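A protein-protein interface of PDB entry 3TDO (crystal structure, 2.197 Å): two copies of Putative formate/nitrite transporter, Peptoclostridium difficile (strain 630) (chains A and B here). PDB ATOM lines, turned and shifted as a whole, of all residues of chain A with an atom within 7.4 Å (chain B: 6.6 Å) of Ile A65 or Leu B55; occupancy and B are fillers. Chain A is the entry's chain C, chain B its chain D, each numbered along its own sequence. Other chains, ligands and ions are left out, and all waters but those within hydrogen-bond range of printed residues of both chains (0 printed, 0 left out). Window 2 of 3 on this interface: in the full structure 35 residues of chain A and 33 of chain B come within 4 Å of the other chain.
Of the 18 printed residues of chain B, 5 touch a printed residue of chain A. Hydrophobic or aromatic side chains of chain B that line the printed part of chain A: Ile B51, Leu B55 and Ala B58. Among the printed residues, 5 pairs touch across the chains. Among the printed residues, no Asp or Glu carboxylate lies within 4 Å of a Lys or Arg side-chain nitrogen of the other chain.
The backbone carbonyl oxygen (O) of Lys A64 sits at hydrogen-bond distance from the side-chain hydroxyl (OG1) of Thr A199 (2.9 Å). The backbone carbonyl oxygen of Phe A195 is in hydrogen-bond range of the side-chain hydroxyl of Thr A199, at 3.2 Å. The backbone carbonyl oxygen (O) of Leu B55 sits at hydrogen-bond distance from the backbone NH (N) of Ser B60 (3.1 Å). OG of Ser B70 is in hydrogen-bond range of O of Val B66, 2.8 Å away.
Printed residues of chain B within 4 Å of Pro A61: Ala B58. Of the printed residues of chain B, Ile A65 touches Leu B55 (3.9 Å). Printed residues of chain B within 4 Å of Phe A195: Ile B51 (3.9 Å) and Ser B70 (3.5 Å). Of the printed residues of chain A, Thr B50 touches Thr A199. Gly B52 touches none of the printed residues of chain A. Printed residues of chain A within 4 Å of Leu B55: Ile A65 (3.9 Å). Thr B56 touches none of the printed residues of chain A. The nearest residue of chain A that does not touch Leu B55 is Met A62 (4.03 Å). The nearest printed residue of chain A that does not touch Ser B70 is Ile A65 (5.5 Å).
Positions printed for both chains: 51, 55, 60, 61, 62, 63, 64, 66, 67 and 70. Of the 5 pairs that touch across the chains among the printed residues, none has its exchanged pair printed and touching as well.
Ala B58 touches Pro A61 (CB to CB, 3.5 Å). Ile A65 touches Leu B55. Ile B51 touches Phe A195. Ser B70 touches Phe A195. Thr B50 touches Thr A199.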
ATOM      1  N   ILE A  51     -13.594   5.701  -9.363  1.00  0.00           N
ATOM      2  CA  ILE A  51     -13.225   6.168  -8.039  1.00  0.00           C
ATOM      3  C   ILE A  51     -13.593   5.151  -6.962  1.00  0.00           C
ATOM      4  O   ILE A  51     -12.822   4.920  -6.031  1.00  0.00           O
ATOM      5  CB  ILE A  51     -13.879   7.538  -7.752  1.00  0.00           C
ATOM      6  CG1 ILE A  51     -13.283   8.585  -8.702  1.00  0.00           C
ATOM      7  CG2 ILE A  51     -13.708   7.926  -6.284  1.00  0.00           C
ATOM      8  CD1 ILE A  51     -13.906   9.957  -8.621  1.00  0.00           C
ATOM      9  N   LEU A  55     -10.808   3.610  -4.623  1.00  0.00           N
ATOM     10  CA  LEU A  55     -10.831   3.863  -3.181  1.00  0.00           C
ATOM     11  C   LEU A  55     -11.240   2.651  -2.350  1.00  0.00           C
ATOM     12  O   LEU A  55     -10.751   2.470  -1.233  1.00  0.00           O
ATOM     13  CB  LEU A  55     -11.689   5.084  -2.855  1.00  0.00           C
ATOM     14  CG  LEU A  55     -11.080   6.386  -3.398  1.00  0.00           C
ATOM     15  CD1 LEU A  55     -11.808   7.583  -2.836  1.00  0.00           C
ATOM     16  CD2 LEU A  55      -9.580   6.480  -3.085  1.00  0.00           C
ATOM     17  N   SER A  60     -10.514   3.087   1.775  1.00  0.00           N
ATOM     18  CA  SER A  60     -10.689   4.452   2.243  1.00  0.00           C
ATOM     19  C   SER A  60     -12.074   4.643   2.859  1.00  0.00           C
ATOM     20  O   SER A  60     -13.065   4.127   2.342  1.00  0.00           O
ATOM     21  CB  SER A  60     -10.479   5.441   1.083  1.00  0.00           C
ATOM     22  OG  SER A  60     -10.473   6.777   1.554  1.00  0.00           O
ATOM     23  N   PRO A  61     -12.147   5.366   3.984  1.00  0.00           N
ATOM     24  CA  PRO A  61     -13.462   5.701   4.537  1.00  0.00           C
ATOM     25  C   PRO A  61     -14.164   6.779   3.688  1.00  0.00           C
ATOM     26  O   PRO A  61     -15.380   6.928   3.775  1.00  0.00           O
ATOM     27  CB  PRO A  61     -13.129   6.210   5.942  1.00  0.00           C
ATOM     28  CG  PRO A  61     -11.772   6.819   5.797  1.00  0.00           C
ATOM     29  CD  PRO A  61     -11.051   6.024   4.719  1.00  0.00           C
ATOM     30  N   MET A  62     -13.395   7.487   2.860  1.00  0.00           N
ATOM     31  CA  MET A  62     -13.883   8.635   2.095  1.00  0.00           C
ATOM     32  C   MET A  62     -14.506   8.254   0.741  1.00  0.00           C
ATOM     33  O   MET A  62     -15.032   9.106   0.021  1.00  0.00           O
ATOM     34  CB  MET A  62     -12.734   9.629   1.884  1.00  0.00           C
ATOM     35  CG  MET A  62     -12.315  10.364   3.144  1.00  0.00           C
ATOM     36  SD  MET A  62     -13.386  11.783   3.520  1.00  0.00           S
ATOM     37  CE  MET A  62     -13.152  12.797   2.053  1.00  0.00           C
ATOM     38  N   THR A  63     -14.455   6.965   0.424  1.00  0.00           N
ATOM     39  CA  THR A  63     -14.909   6.425  -0.847  1.00  0.00           C
ATOM     40  C   THR A  63     -16.256   7.006  -1.321  1.00  0.00           C
ATOM     41  O   THR A  63     -16.356   7.616  -2.404  1.00  0.00           O
ATOM     42  CB  THR A  63     -14.996   4.888  -0.720  1.00  0.00           C
ATOM     43  OG1 THR A  63     -13.689   4.378  -0.429  1.00  0.00           O
ATOM     44  CG2 THR A  63     -15.530   4.238  -1.981  1.00  0.00           C
ATOM     45  N   LYS A  64     -17.293   6.785  -0.521  1.00  0.00           N
ATOM     46  CA  LYS A  64     -18.642   7.223  -0.856  1.00  0.00           C
ATOM     47  C   LYS A  64     -18.809   8.745  -0.890  1.00  0.00           C
ATOM     48  O   LYS A  64     -19.711   9.252  -1.545  1.00  0.00           O
ATOM     49  CB  LYS A  64     -19.652   6.610   0.109  1.00  0.00           C
ATOM     50  CG  LYS A  64     -19.830   5.102  -0.054  1.00  0.00           C
ATOM     51  CD  LYS A  64     -20.798   4.552   0.984  1.00  0.00           C
ATOM     52  CE  LYS A  64     -20.832   3.011   1.013  1.00  0.00           C
ATOM     53  NZ  LYS A  64     -21.442   2.421  -0.217  1.00  0.00           N
ATOM     54  N   ILE A  65     -17.963   9.469  -0.166  1.00  0.00           N
ATOM     55  CA  ILE A  65     -18.051  10.934  -0.163  1.00  0.00           C
ATOM     56  C   ILE A  65     -17.471  11.496  -1.449  1.00  0.00           C
ATOM     57  O   ILE A  65     -18.081  12.326  -2.129  1.00  0.00           O
ATOM     58  CB  ILE A  65     -17.337  11.521   1.075  1.00  0.00           C
ATOM     59  CG1 ILE A  65     -17.994  10.957   2.346  1.00  0.00           C
ATOM     60  CG2 ILE A  65     -17.355  13.072   1.041  1.00  0.00           C
ATOM     61  CD1 ILE A  65     -17.142  11.042   3.607  1.00  0.00           C
ATOM     62  N   VAL A  66     -16.295  10.997  -1.805  1.00  0.00           N
ATOM     63  CA  VAL A  66     -15.646  11.376  -3.041  1.00  0.00           C
ATOM     64  C   VAL A  66     -16.531  11.025  -4.253  1.00  0.00           C
ATOM     65  O   VAL A  66     -16.699  11.834  -5.169  1.00  0.00           O
ATOM     66  CB  VAL A  66     -14.231  10.741  -3.084  1.00  0.00           C
ATOM     67  CG1 VAL A  66     -13.442  11.189  -4.295  1.00  0.00           C
ATOM     68  CG2 VAL A  66     -13.488  11.123  -1.811  1.00  0.00           C
ATOM     69  N   MET A  67     -17.153   9.852  -4.226  1.00  0.00           N
ATOM     70  CA  MET A  67     -18.037   9.460  -5.311  1.00  0.00           C
ATOM     71  C   MET A  67     -19.171  10.458  -5.490  1.00  0.00           C
ATOM     72  O   MET A  67     -19.445  10.897  -6.607  1.00  0.00           O
ATOM     73  CB  MET A  67     -18.616   8.059  -5.069  1.00  0.00           C
ATOM     74  CG  MET A  67     -17.616   6.934  -5.274  1.00  0.00           C
ATOM     75  SD  MET A  67     -18.314   5.308  -4.875  1.00  0.00           S
ATOM     76  CE  MET A  67     -19.555   5.121  -6.148  1.00  0.00           C
ATOM     77  N   GLY A  68     -19.835  10.809  -4.392  1.00  0.00           N
ATOM     78  CA  GLY A  68     -20.922  11.770  -4.472  1.00  0.00           C
ATOM     79  C   GLY A  68     -20.427  13.126  -4.944  1.00  0.00           C
ATOM     80  O   GLY A  68     -21.015  13.742  -5.848  1.00  0.00           O
ATOM     81  N   LEU A  69     -19.319  13.583  -4.365  1.00  0.00           N
ATOM     82  CA  LEU A  69     -18.734  14.866  -4.790  1.00  0.00           C
ATOM     83  C   LEU A  69     -18.409  14.874  -6.276  1.00  0.00           C
ATOM     84  O   LEU A  69     -18.351  15.931  -6.895  1.00  0.00           O
ATOM     85  CB  LEU A  69     -17.466  15.196  -3.994  1.00  0.00           C
ATOM     86  CG  LEU A  69     -17.644  15.554  -2.506  1.00  0.00           C
ATOM     87  CD1 LEU A  69     -16.271  15.549  -1.794  1.00  0.00           C
ATOM     88  CD2 LEU A  69     -18.343  16.912  -2.363  1.00  0.00           C
ATOM     89  N   SER A  70     -18.182  13.691  -6.843  1.00  0.00           N
ATOM     90  CA  SER A  70     -17.701  13.586  -8.223  1.00  0.00           C
ATOM     91  C   SER A  70     -18.769  13.298  -9.259  1.00  0.00           C
ATOM     92  O   SER A  70     -18.452  13.153 -10.440  1.00  0.00           O
ATOM     93  CB  SER A  70     -16.583  12.535  -8.337  1.00  0.00           C
ATOM     94  OG  SER A  70     -15.536  12.839  -7.437  1.00  0.00           O
ATOM     95  N   PHE A  71     -20.026  13.211  -8.836  1.00  0.00           N
ATOM     96  CA  PHE A  71     -21.099  12.815  -9.761  1.00  0.00           C
ATOM     97  C   PHE A  71     -21.785  13.967 -10.513  1.00  0.00           C
ATOM     98  O   PHE A  71     -22.579  13.725 -11.437  1.00  0.00           O
ATOM     99  CB  PHE A  71     -22.150  11.995  -9.013  1.00  0.00           C
ATOM    100  CG  PHE A  71     -23.062  11.213  -9.916  1.00  0.00           C
ATOM    101  CD1 PHE A  71     -22.536  10.365 -10.879  1.00  0.00           C
ATOM    102  CD2 PHE A  71     -24.445  11.304  -9.787  1.00  0.00           C
ATOM    103  CE1 PHE A  71     -23.372   9.620 -11.713  1.00  0.00           C
ATOM    104  CE2 PHE A  71     -25.284  10.563 -10.609  1.00  0.00           C
ATOM    105  CZ  PHE A  71     -24.742   9.718 -11.576  1.00  0.00           C
ATOM    106  N   PHE A 195     -24.481  15.100  -5.046  1.00  0.00           N
ATOM    107  CA  PHE A 195     -23.621  14.725  -3.928  1.00  0.00           C
ATOM    108  C   PHE A 195     -24.525  14.113  -2.834  1.00  0.00           C
ATOM    109  O   PHE A 195     -24.270  13.012  -2.323  1.00  0.00           O
ATOM    110  CB  PHE A 195     -22.885  15.991  -3.421  1.00  0.00           C
ATOM    111  CG  PHE A 195     -22.077  15.796  -2.151  1.00  0.00           C
ATOM    112  CD1 PHE A 195     -21.653  14.528  -1.738  1.00  0.00           C
ATOM    113  CD2 PHE A 195     -21.732  16.902  -1.374  1.00  0.00           C
ATOM    114  CE1 PHE A 195     -20.883  14.376  -0.568  1.00  0.00           C
ATOM    115  CE2 PHE A 195     -20.987  16.758  -0.203  1.00  0.00           C
ATOM    116  CZ  PHE A 195     -20.558  15.500   0.195  1.00  0.00           C
ATOM    117  N   ILE A 198     -26.101  10.617  -4.300  1.00  0.00           N
ATOM    118  CA  ILE A 198     -25.118   9.535  -4.404  1.00  0.00           C
ATOM    119  C   ILE A 198     -24.587   9.088  -3.030  1.00  0.00           C
ATOM    120  O   ILE A 198     -24.596   7.907  -2.716  1.00  0.00           O
ATOM    121  CB  ILE A 198     -23.935   9.905  -5.332  1.00  0.00           C
ATOM    122  CG1 ILE A 198     -24.383   9.901  -6.800  1.00  0.00           C
ATOM    123  CG2 ILE A 198     -22.777   8.916  -5.140  1.00  0.00           C
ATOM    124  CD1 ILE A 198     -24.844   8.531  -7.317  1.00  0.00           C
ATOM    125  N   THR A 199     -24.127  10.031  -2.212  1.00  0.00           N
ATOM    126  CA  THR A 199     -23.515   9.679  -0.934  1.00  0.00           C
ATOM    127  C   THR A 199     -24.532   9.101   0.076  1.00  0.00           C
ATOM    128  O   THR A 199     -24.226   8.157   0.801  1.00  0.00           O
ATOM    129  CB  THR A 199     -22.743  10.877  -0.340  1.00  0.00           C
ATOM    130  OG1 THR A 199     -21.753  11.301  -1.287  1.00  0.00           O
ATOM    131  CG2 THR A 199     -22.063  10.494   0.981  1.00  0.00           C
ATOM    132  N   THR B  50     -24.978  10.685   7.132  1.00  0.00           N
ATOM    133  CA  THR B  50     -24.342   9.559   6.438  1.00  0.00           C
ATOM    134  C   THR B  50     -22.822   9.713   6.520  1.00  0.00           C
ATOM    135  O   THR B  50     -22.104   8.775   6.838  1.00  0.00           O
ATOM    136  CB  THR B  50     -24.807   9.478   4.973  1.00  0.00           C
ATOM    137  OG1 THR B  50     -26.226   9.287   4.948  1.00  0.00           O
ATOM    138  CG2 THR B  50     -24.136   8.317   4.231  1.00  0.00           C
ATOM    139  N   ILE B  51     -22.362  10.931   6.246  1.00  0.00           N
ATOM    140  CA  ILE B  51     -20.972  11.336   6.404  1.00  0.00           C
ATOM    141  C   ILE B  51     -20.569  11.147   7.867  1.00  0.00           C
ATOM    142  O   ILE B  51     -19.543  10.539   8.166  1.00  0.00           O
ATOM    143  CB  ILE B  51     -20.809  12.830   5.953  1.00  0.00           C
ATOM    144  CG1 ILE B  51     -20.810  12.915   4.424  1.00  0.00           C
ATOM    145  CG2 ILE B  51     -19.551  13.472   6.547  1.00  0.00           C
ATOM    146  CD1 ILE B  51     -21.097  14.271   3.877  1.00  0.00           C
ATOM    147  N   GLY B  52     -21.396  11.645   8.785  1.00  0.00           N
ATOM    148  CA  GLY B  52     -21.128  11.472  10.207  1.00  0.00           C
ATOM    149  C   GLY B  52     -20.877  10.013  10.576  1.00  0.00           C
ATOM    150  O   GLY B  52     -19.879   9.665  11.216  1.00  0.00           O
ATOM    151  N   GLY B  53     -21.791   9.141  10.162  1.00  0.00           N
ATOM    152  CA  GLY B  53     -21.623   7.723  10.427  1.00  0.00           C
ATOM    153  C   GLY B  53     -20.342   7.175   9.828  1.00  0.00           C
ATOM    154  O   GLY B  53     -19.557   6.517  10.517  1.00  0.00           O
ATOM    155  N   LEU B  54     -20.139   7.433   8.537  1.00  0.00           N
ATOM    156  CA  LEU B  54     -18.978   6.893   7.825  1.00  0.00           C
ATOM    157  C   LEU B  54     -17.647   7.315   8.453  1.00  0.00           C
ATOM    158  O   LEU B  54     -16.774   6.486   8.693  1.00  0.00           O
ATOM    159  CB  LEU B  54     -19.017   7.284   6.334  1.00  0.00           C
ATOM    160  CG  LEU B  54     -20.072   6.624   5.438  1.00  0.00           C
ATOM    161  CD1 LEU B  54     -20.240   7.447   4.162  1.00  0.00           C
ATOM    162  CD2 LEU B  54     -19.751   5.128   5.120  1.00  0.00           C
ATOM    163  N   LEU B  55     -17.491   8.605   8.732  1.00  0.00           N
ATOM    164  CA  LEU B  55     -16.208   9.102   9.240  1.00  0.00           C
ATOM    165  C   LEU B  55     -16.013   8.832  10.742  1.00  0.00           C
ATOM    166  O   LEU B  55     -14.904   8.623  11.197  1.00  0.00           O
ATOM    167  CB  LEU B  55     -16.070  10.599   8.939  1.00  0.00           C
ATOM    168  CG  LEU B  55     -16.029  10.933   7.433  1.00  0.00           C
ATOM    169  CD1 LEU B  55     -15.650  12.388   7.191  1.00  0.00           C
ATOM    170  CD2 LEU B  55     -15.064  10.006   6.727  1.00  0.00           C
ATOM    171  N   THR B  56     -17.091   8.891  11.516  1.00  0.00           N
ATOM    172  CA  THR B  56     -17.019   8.484  12.922  1.00  0.00           C
ATOM    173  C   THR B  56     -16.513   7.051  13.040  1.00  0.00           C
ATOM    174  O   THR B  56     -15.631   6.741  13.868  1.00  0.00           O
ATOM    175  CB  THR B  56     -18.403   8.606  13.606  1.00  0.00           C
ATOM    176  OG1 THR B  56     -18.760   9.989  13.700  1.00  0.00           O
ATOM    177  CG2 THR B  56     -18.395   7.985  14.997  1.00  0.00           C
ATOM    178  N   ASP B  57     -17.067   6.167  12.214  1.00  0.00           N
ATOM    179  CA  ASP B  57     -16.702   4.737  12.276  1.00  0.00           C
ATOM    180  C   ASP B  57     -15.243   4.551  11.865  1.00  0.00           C
ATOM    181  O   ASP B  57     -14.630   3.525  12.143  1.00  0.00           O
ATOM    182  CB  ASP B  57     -17.638   3.907  11.381  1.00  0.00           C
ATOM    183  CG  ASP B  57     -17.532   2.408  11.627  1.00  0.00           C
ATOM    184  OD1 ASP B  57     -17.610   1.964  12.799  1.00  0.00           O
ATOM    185  OD2 ASP B  57     -17.379   1.667  10.632  1.00  0.00           O
ATOM    186  N   ALA B  58     -14.689   5.560  11.202  1.00  0.00           N
ATOM    187  CA  ALA B  58     -13.302   5.519  10.748  1.00  0.00           C
ATOM    188  C   ALA B  58     -12.338   6.133  11.762  1.00  0.00           C
ATOM    189  O   ALA B  58     -11.117   6.011  11.630  1.00  0.00           O
ATOM    190  CB  ALA B  58     -13.180   6.228   9.399  1.00  0.00           C
ATOM    191  N   GLY B  59     -12.885   6.782  12.782  1.00  0.00           N
ATOM    192  CA  GLY B  59     -12.066   7.525  13.726  1.00  0.00           C
ATOM    193  C   GLY B  59     -11.474   8.821  13.175  1.00  0.00           C
ATOM    194  O   GLY B  59     -10.536   9.360  13.745  1.00  0.00           O
ATOM    195  N   SER B  60     -12.016   9.350  12.084  1.00  0.00           N
ATOM    196  CA  SER B  60     -11.417  10.549  11.479  1.00  0.00           C
ATOM    197  C   SER B  60     -11.574  11.835  12.305  1.00  0.00           C
ATOM    198  O   SER B  60     -12.655  12.144  12.809  1.00  0.00           O
ATOM    199  CB  SER B  60     -11.943  10.785  10.060  1.00  0.00           C
ATOM    200  OG  SER B  60     -11.844  12.161   9.713  1.00  0.00           O
ATOM    201  N   PRO B  61     -10.484  12.598  12.430  1.00  0.00           N
ATOM    202  CA  PRO B  61     -10.520  13.938  13.026  1.00  0.00           C
ATOM    203  C   PRO B  61     -11.300  14.934  12.165  1.00  0.00           C
ATOM    204  O   PRO B  61     -11.663  15.998  12.659  1.00  0.00           O
ATOM    205  CB  PRO B  61      -9.039  14.332  13.088  1.00  0.00           C
ATOM    206  CG  PRO B  61      -8.380  13.497  12.037  1.00  0.00           C
ATOM    207  CD  PRO B  61      -9.122  12.201  12.034  1.00  0.00           C
ATOM    208  N   MET B  62     -11.563  14.591  10.905  1.00  0.00           N
ATOM    209  CA  MET B  62     -12.217  15.520   9.976  1.00  0.00           C
ATOM    210  C   MET B  62     -13.750  15.449   9.976  1.00  0.00           C
ATOM    211  O   MET B  62     -14.408  16.260   9.323  1.00  0.00           O
ATOM    212  CB  MET B  62     -11.664  15.313   8.553  1.00  0.00           C
ATOM    213  CG  MET B  62     -10.193  15.723   8.425  1.00  0.00           C
ATOM    214  SD  MET B  62      -9.976  17.529   8.470  1.00  0.00           S
ATOM    215  CE  MET B  62     -10.744  17.983   6.920  1.00  0.00           C
ATOM    216  N   THR B  63     -14.314  14.508  10.736  1.00  0.00           N
ATOM    217  CA  THR B  63     -15.764  14.255  10.736  1.00  0.00           C
ATOM    218  C   THR B  63     -16.613  15.543  10.758  1.00  0.00           C
ATOM    219  O   THR B  63     -17.375  15.807   9.832  1.00  0.00           O
ATOM    220  CB  THR B  63     -16.196  13.332  11.922  1.00  0.00           C
ATOM    221  OG1 THR B  63     -15.559  12.061  11.787  1.00  0.00           O
ATOM    222  CG2 THR B  63     -17.714  13.115  11.929  1.00  0.00           C
ATOM    223  N   LYS B  64     -16.486  16.331  11.818  1.00  0.00           N
ATOM    224  CA  LYS B  64     -17.339  17.495  12.002  1.00  0.00           C
ATOM    225  C   LYS B  64     -17.058  18.592  10.982  1.00  0.00           C
ATOM    226  O   LYS B  64     -17.939  19.374  10.656  1.00  0.00           O
ATOM    227  CB  LYS B  64     -17.243  18.020  13.437  1.00  0.00           C
ATOM    228  CG  LYS B  64     -17.824  17.024  14.465  1.00  0.00           C
ATOM    229  CD  LYS B  64     -17.667  17.509  15.897  1.00  0.00           C
ATOM    230  CE  LYS B  64     -18.338  16.573  16.906  1.00  0.00           C
ATOM    231  NZ  LYS B  64     -18.021  17.041  18.266  1.00  0.00           N
ATOM    232  N   VAL B  66     -16.048  17.998   7.735  1.00  0.00           N
ATOM    233  CA  VAL B  66     -16.672  17.531   6.506  1.00  0.00           C
ATOM    234  C   VAL B  66     -18.205  17.631   6.584  1.00  0.00           C
ATOM    235  O   VAL B  66     -18.856  17.993   5.603  1.00  0.00           O
ATOM    236  CB  VAL B  66     -16.232  16.083   6.160  1.00  0.00           C
ATOM    237  CG1 VAL B  66     -16.925  15.615   4.887  1.00  0.00           C
ATOM    238  CG2 VAL B  66     -14.696  16.010   6.006  1.00  0.00           C
ATOM    239  N   MET B  67     -18.781  17.315   7.746  1.00  0.00           N
ATOM    240  CA  MET B  67     -20.213  17.493   7.938  1.00  0.00           C
ATOM    241  C   MET B  67     -20.588  18.951   7.677  1.00  0.00           C
ATOM    242  O   MET B  67     -21.524  19.228   6.920  1.00  0.00           O
ATOM    243  CB  MET B  67     -20.646  17.064   9.343  1.00  0.00           C
ATOM    244  CG  MET B  67     -20.656  15.552   9.556  1.00  0.00           C
ATOM    245  SD  MET B  67     -21.023  15.087  11.256  1.00  0.00           S
ATOM    246  CE  MET B  67     -22.779  15.514  11.409  1.00  0.00           C
ATOM    247  N   SER B  70     -20.552  19.977   4.157  1.00  0.00           N
ATOM    248  CA  SER B  70     -21.496  19.254   3.330  1.00  0.00           C
ATOM    249  C   SER B  70     -22.969  19.616   3.548  1.00  0.00           C
ATOM    250  O   SER B  70     -23.848  18.979   2.959  1.00  0.00           O
ATOM    251  CB  SER B  70     -21.249  17.742   3.488  1.00  0.00           C
ATOM    252  OG  SER B  70     -19.911  17.454   3.066  1.00  0.00           O
